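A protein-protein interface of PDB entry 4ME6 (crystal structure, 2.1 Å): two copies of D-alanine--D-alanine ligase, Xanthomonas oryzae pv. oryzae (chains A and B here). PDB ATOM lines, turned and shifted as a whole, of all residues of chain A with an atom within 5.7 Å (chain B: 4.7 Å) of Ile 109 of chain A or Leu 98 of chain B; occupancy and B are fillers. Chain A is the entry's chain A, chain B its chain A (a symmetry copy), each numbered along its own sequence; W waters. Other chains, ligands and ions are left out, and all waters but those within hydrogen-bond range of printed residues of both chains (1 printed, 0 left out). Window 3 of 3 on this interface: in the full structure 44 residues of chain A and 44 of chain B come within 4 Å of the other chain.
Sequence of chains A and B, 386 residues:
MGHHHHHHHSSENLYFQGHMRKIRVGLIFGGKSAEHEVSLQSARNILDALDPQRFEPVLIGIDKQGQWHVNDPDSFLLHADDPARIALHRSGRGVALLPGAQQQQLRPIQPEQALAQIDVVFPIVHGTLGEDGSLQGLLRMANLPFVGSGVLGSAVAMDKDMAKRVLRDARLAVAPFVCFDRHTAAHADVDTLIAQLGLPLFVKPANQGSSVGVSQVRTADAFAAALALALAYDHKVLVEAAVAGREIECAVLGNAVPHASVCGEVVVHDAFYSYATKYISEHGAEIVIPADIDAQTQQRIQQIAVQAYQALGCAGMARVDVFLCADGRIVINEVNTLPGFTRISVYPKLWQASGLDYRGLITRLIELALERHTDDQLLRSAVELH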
ATOM      1  N   ARG A  93      10.212   3.783 -13.166  1.00  0.00           N
ATOM      2  CA  ARG A  93      10.706   5.004 -12.565  1.00  0.00           C
ATOM      3  C   ARG A  93      12.073   4.716 -11.951  1.00  0.00           C
ATOM      4  O   ARG A  93      12.182   4.197 -10.828  1.00  0.00           O
ATOM      5  CB  ARG A  93       9.751   5.448 -11.475  1.00  0.00           C
ATOM      6  CG  ARG A  93       8.350   5.674 -12.029  1.00  0.00           C
ATOM      7  CD  ARG A  93       7.360   5.612 -10.915  1.00  0.00           C
ATOM      8  NE  ARG A  93       7.638   6.621  -9.913  1.00  0.00           N
ATOM      9  CZ  ARG A  93       6.971   6.715  -8.767  1.00  0.00           C
ATOM     10  NH1 ARG A  93       6.026   5.824  -8.486  1.00  0.00           N
ATOM     11  NH2 ARG A  93       7.255   7.689  -7.891  1.00  0.00           N
ATOM     12  N   GLY A  94      13.110   5.052 -12.702  1.00  0.00           N
ATOM     13  CA  GLY A  94      14.447   4.637 -12.395  1.00  0.00           C
ATOM     14  C   GLY A  94      15.045   5.479 -11.311  1.00  0.00           C
ATOM     15  O   GLY A  94      14.533   6.572 -11.012  1.00  0.00           O
ATOM     16  N   VAL A  95      16.135   4.965 -10.749  1.00  0.00           N
ATOM     17  CA  VAL A  95      16.860   5.609  -9.638  1.00  0.00           C
ATOM     18  C   VAL A  95      18.322   5.864  -9.977  1.00  0.00           C
ATOM     19  O   VAL A  95      19.015   4.966 -10.434  1.00  0.00           O
ATOM     20  CB  VAL A  95      16.853   4.748  -8.356  1.00  0.00           C
ATOM     21  CG1 VAL A  95      17.273   5.567  -7.170  1.00  0.00           C
ATOM     22  CG2 VAL A  95      15.481   4.164  -8.067  1.00  0.00           C
ATOM     23  N   ALA A  96      18.787   7.081  -9.719  1.00  0.00           N
ATOM     24  CA  ALA A  96      20.196   7.434  -9.786  1.00  0.00           C
ATOM     25  C   ALA A  96      20.722   7.692  -8.387  1.00  0.00           C
ATOM     26  O   ALA A  96      20.037   8.232  -7.538  1.00  0.00           O
ATOM     27  CB  ALA A  96      20.417   8.680 -10.643  1.00  0.00           C
ATOM     28  N   LEU A  97      21.957   7.297  -8.174  1.00  0.00           N
ATOM     29  CA  LEU A  97      22.650   7.557  -6.956  1.00  0.00           C
ATOM     30  C   LEU A  97      23.725   8.639  -7.167  1.00  0.00           C
ATOM     31  O   LEU A  97      24.456   8.647  -8.170  1.00  0.00           O
ATOM     32  CB  LEU A  97      23.299   6.255  -6.522  1.00  0.00           C
ATOM     33  CG  LEU A  97      23.760   6.355  -5.089  1.00  0.00           C
ATOM     34  CD1 LEU A  97      22.655   5.685  -4.275  1.00  0.00           C
ATOM     35  CD2 LEU A  97      25.126   5.707  -4.902  1.00  0.00           C
ATOM     36  N   ARG A 107      18.084   9.830  -6.586  1.00  0.00           N
ATOM     37  CA  ARG A 107      17.552  10.831  -7.504  1.00  0.00           C
ATOM     38  C   ARG A 107      16.705  10.072  -8.476  1.00  0.00           C
ATOM     39  O   ARG A 107      17.049   8.975  -8.854  1.00  0.00           O
ATOM     40  CB  ARG A 107      18.702  11.454  -8.281  1.00  0.00           C
ATOM     41  CG  ARG A 107      18.654  12.952  -8.448  1.00  0.00           C
ATOM     42  CD  ARG A 107      19.051  13.671  -7.155  1.00  0.00           C
ATOM     43  NE  ARG A 107      19.497  15.022  -7.452  1.00  0.00           N
ATOM     44  CZ  ARG A 107      20.211  15.801  -6.651  1.00  0.00           C
ATOM     45  NH1 ARG A 107      20.583  15.407  -5.448  1.00  0.00           N
ATOM     46  NH2 ARG A 107      20.550  17.008  -7.068  1.00  0.00           N
ATOM     47  N   PRO A 108      15.594  10.646  -8.903  1.00  0.00           N
ATOM     48  CA  PRO A 108      14.798   9.955  -9.878  1.00  0.00           C
ATOM     49  C   PRO A 108      15.389  10.156 -11.233  1.00  0.00           C
ATOM     50  O   PRO A 108      15.683  11.271 -11.598  1.00  0.00           O
ATOM     51  CB  PRO A 108      13.453  10.687  -9.803  1.00  0.00           C
ATOM     52  CG  PRO A 108      13.829  12.061  -9.402  1.00  0.00           C
ATOM     53  CD  PRO A 108      14.955  11.884  -8.435  1.00  0.00           C
ATOM     54  N   ILE A 109      15.573   9.087 -11.976  1.00  0.00           N
ATOM     55  CA  ILE A 109      15.911   9.219 -13.374  1.00  0.00           C
ATOM     56  C   ILE A 109      14.635   9.704 -14.056  1.00  0.00           C
ATOM     57  O   ILE A 109      13.553   9.155 -13.781  1.00  0.00           O
ATOM     58  CB  ILE A 109      16.310   7.882 -13.973  1.00  0.00           C
ATOM     59  CG1 ILE A 109      17.586   7.363 -13.309  1.00  0.00           C
ATOM     60  CG2 ILE A 109      16.488   8.028 -15.473  1.00  0.00           C
ATOM     61  CD1 ILE A 109      17.890   5.927 -13.668  1.00  0.00           C
ATOM     62  N   GLN A 110      14.760  10.719 -14.917  1.00  0.00           N
ATOM     63  CA  GLN A 110      13.615  11.361 -15.576  1.00  0.00           C
ATOM     64  C   GLN A 110      12.733  12.126 -14.583  1.00  0.00           C
ATOM     65  O   GLN A 110      13.215  13.019 -13.885  1.00  0.00           O
ATOM     66  CB  GLN A 110      12.803  10.338 -16.390  1.00  0.00           C
ATOM     67  CG  GLN A 110      11.565   9.755 -15.698  1.00  0.00           C
ATOM     68  CD  GLN A 110      11.438   8.237 -15.867  1.00  0.00           C
ATOM     69  OE1 GLN A 110      12.432   7.511 -15.891  1.00  0.00           O
ATOM     70  NE2 GLN A 110      10.205   7.755 -15.962  1.00  0.00           N
ATOM     71  N   ALA B  96      26.490  10.847 -11.645  1.00  0.00           N
ATOM     72  CA  ALA B  96      25.446   9.982 -11.122  1.00  0.00           C
ATOM     73  C   ALA B  96      25.764   8.538 -11.464  1.00  0.00           C
ATOM     74  O   ALA B  96      26.281   8.234 -12.523  1.00  0.00           O
ATOM     75  CB  ALA B  96      24.080  10.346 -11.699  1.00  0.00           C
ATOM     76  N   LEU B  97      25.435   7.661 -10.543  1.00  0.00           N
ATOM     77  CA  LEU B  97      25.557   6.255 -10.738  1.00  0.00           C
ATOM     78  C   LEU B  97      24.170   5.613 -10.919  1.00  0.00           C
ATOM     79  O   LEU B  97      23.202   5.936 -10.211  1.00  0.00           O
ATOM     80  CB  LEU B  97      26.239   5.687  -9.506  1.00  0.00           C
ATOM     81  CG  LEU B  97      26.709   4.279  -9.775  1.00  0.00           C
ATOM     82  CD1 LEU B  97      28.191   4.420 -10.116  1.00  0.00           C
ATOM     83  CD2 LEU B  97      26.449   3.374  -8.577  1.00  0.00           C
ATOM     84  N   LEU B  98      24.049   4.751 -11.897  1.00  0.00           N
ATOM     85  CA  LEU B  98      22.823   4.031 -12.114  1.00  0.00           C
ATOM     86  C   LEU B  98      22.896   2.593 -11.650  1.00  0.00           C
ATOM     87  O   LEU B  98      23.314   1.729 -12.391  1.00  0.00           O
ATOM     88  CB  LEU B  98      22.463   4.082 -13.568  1.00  0.00           C
ATOM     89  CG  LEU B  98      21.674   5.346 -13.919  1.00  0.00           C
ATOM     90  CD1 LEU B  98      22.281   6.591 -13.339  1.00  0.00           C
ATOM     91  CD2 LEU B  98      21.509   5.444 -15.413  1.00  0.00           C
ATOM     92  N   PRO B  99      22.464   2.321 -10.414  1.00  0.00           N
ATOM     93  CA  PRO B  99      22.608   0.946  -9.907  1.00  0.00           C
ATOM     94  C   PRO B  99      21.721   0.017 -10.648  1.00  0.00           C
ATOM     95  O   PRO B  99      20.626   0.391 -10.981  1.00  0.00           O
ATOM     96  CB  PRO B  99      22.190   1.041  -8.437  1.00  0.00           C
ATOM     97  CG  PRO B  99      21.514   2.372  -8.284  1.00  0.00           C
ATOM     98  CD  PRO B  99      22.038   3.257  -9.360  1.00  0.00           C
ATOM     99  N   GLY B 100      22.238  -1.165 -10.961  1.00  0.00           N
ATOM    100  CA  GLY B 100      21.507  -2.126 -11.773  1.00  0.00           C
ATOM    101  C   GLY B 100      21.644  -1.904 -13.269  1.00  0.00           C
ATOM    102  O   GLY B 100      21.289  -2.763 -14.046  1.00  0.00           O
ATOM    103  N   ALA B 101      22.188  -0.769 -13.687  1.00  0.00           N
ATOM    104  CA  ALA B 101      22.322  -0.501 -15.101  1.00  0.00           C
ATOM    105  C   ALA B 101      23.478  -1.338 -15.624  1.00  0.00           C
ATOM    106  O   ALA B 101      24.408  -1.682 -14.863  1.00  0.00           O
ATOM    107  CB  ALA B 101      22.559   0.985 -15.348  1.00  0.00           C
ATOM    108  N   GLN B 104      26.261   2.686 -19.764  1.00  0.00           N
ATOM    109  CA  GLN B 104      26.253   4.080 -19.307  1.00  0.00           C
ATOM    110  C   GLN B 104      25.926   4.206 -17.795  1.00  0.00           C
ATOM    111  O   GLN B 104      25.113   5.035 -17.378  1.00  0.00           O
ATOM    112  CB  GLN B 104      25.245   4.911 -20.140  1.00  0.00           C
ATOM    113  CG  GLN B 104      25.770   5.382 -21.479  1.00  0.00           C
ATOM    114  CD  GLN B 104      26.777   6.499 -21.299  1.00  0.00           C
ATOM    115  OE1 GLN B 104      26.634   7.354 -20.421  1.00  0.00           O
ATOM    116  NE2 GLN B 104      27.815   6.477 -22.089  1.00  0.00           N
ATOM    117  N   GLN B 105      26.591   3.394 -16.982  1.00  0.00           N
ATOM    118  CA  GLN B 105      26.298   3.339 -15.555  1.00  0.00           C
ATOM    119  C   GLN B 105      26.705   4.567 -14.835  1.00  0.00           C
ATOM    120  O   GLN B 105      26.076   4.932 -13.841  1.00  0.00           O
ATOM    121  CB  GLN B 105      26.971   2.167 -14.898  1.00  0.00           C
ATOM    122  CG  GLN B 105      26.662   0.908 -15.590  1.00  0.00           C
ATOM    123  CD  GLN B 105      27.695   0.604 -16.600  1.00  0.00           C
ATOM    124  OE1 GLN B 105      28.031   1.447 -17.418  1.00  0.00           O
ATOM    125  NE2 GLN B 105      28.224  -0.604 -16.549  1.00  0.00           N
ATOM    126  N   ARG B 107      26.910   8.496 -15.132  1.00  0.00           N
ATOM    127  CA  ARG B 107      26.082   9.406 -15.917  1.00  0.00           C
ATOM    128  C   ARG B 107      26.490  10.782 -15.495  1.00  0.00           C
ATOM    129  O   ARG B 107      26.768  11.006 -14.338  1.00  0.00           O
ATOM    130  CB  ARG B 107      24.625   9.215 -15.525  1.00  0.00           C
ATOM    131  CG  ARG B 107      23.633   9.178 -16.660  1.00  0.00           C
ATOM    132  CD  ARG B 107      23.679   7.837 -17.397  1.00  0.00           C
ATOM    133  NE  ARG B 107      22.429   7.614 -18.108  1.00  0.00           N
ATOM    134  CZ  ARG B 107      21.990   6.450 -18.565  1.00  0.00           C
ATOM    135  NH1 ARG B 107      22.689   5.339 -18.427  1.00  0.00           N
ATOM    136  NH2 ARG B 107      20.823   6.406 -19.184  1.00  0.00           N
ATOM    137  N   ALA B 142      27.095  -1.136  -9.844  1.00  0.00           N
ATOM    138  CA  ALA B 142      27.034  -0.583 -11.182  1.00  0.00           C
ATOM    139  C   ALA B 142      27.529  -1.546 -12.251  1.00  0.00           C
ATOM    140  O   ALA B 142      27.725  -1.160 -13.381  1.00  0.00           O
ATOM    141  CB  ALA B 142      27.862   0.696 -11.258  1.00  0.00           C
HETATM  142  O   HOH W   1      19.744   2.923 -11.931  1.00  0.00           O
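Water W1 bridges the backbone carbonyl oxygen (O) of Val 95 of chain A (2.6 Å) and the backbone carbonyl oxygen (O) of Pro 99 of chain B (2.8 Å).
Ala 96 of chain A touches Leu 97 of chain B, and with the chains exchanged Leu 97 of chain A touches Ala 96 of chain B.
Leu 97 of chain B touches its own counterpart, Leu 97 of chain A.
Of the 6 pairs that touch across the chains among the printed residues, 3 have their exchanged pair printed and touching as well.
The backbone NH (N) of Ile 109 of chain A sits at hydrogen-bond distance from the backbone carbonyl oxygen (O) of Gly 94 of chain A (2.9 Å).
The backbone carbonyl oxygen of Ala 96 of chain A sits at hydrogen-bond distance from the backbone NH of Arg 107 of chain A (2.7 Å).
The backbone carbonyl oxygen of Ala 96 of chain B sits at hydrogen-bond distance from the backbone NH of Arg 107 of chain B.
O of Gln 105 of chain B is in hydrogen-bond range of N of Leu 98 of chain B.
Hydrophobic or aromatic side chains of chain B that line the printed part of chain A: Ala 96, Leu 97, Leu 98 and Pro 99.
Of the 9 printed residues of chain A, 4 touch a printed residue of chain B.
Along chain A the printed residues that touch a printed residue of chain B span positions 95 to 109.
Among the printed residues, no Asp or Glu carboxylate lies within 4 Å of a Lys or Arg side-chain nitrogen of the other chain.
Among the printed residues, pairs that only touch across the chains: Ala 96 of chain A with Leu 97 of chain B, Leu 97 of chain A with Ala 96 of chain B, Val 95 of chain A with Pro 99 of chain B, Ile 109 of chain A with Leu 98 of chain B and Ala 96 of chain A with Leu 98 of chain B.
Of the printed residues of chain B, Leu 97 of chain A touches Ala 96 (3.4 Å) and Leu 97 (2.7 Å).
Ile 109 of chain A touches just one residue of chain B: Leu 98.
Of the printed residues of chain A, Leu 97 of chain B touches Ala 96 and Leu 97.
The nearest residue of chain A that does not touch Leu 98 of chain B is Val 95 of chain A (4.3 Å).
The nearest printed residue of chain A that does not touch Pro 99 of chain B is Leu 97 of chain A (4.2 Å).
The backbone NH (N) of Leu 97 of chain A sits at hydrogen-bond distance from the backbone carbonyl oxygen (O) of Leu 97 of chain B, at 2.7 Å.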
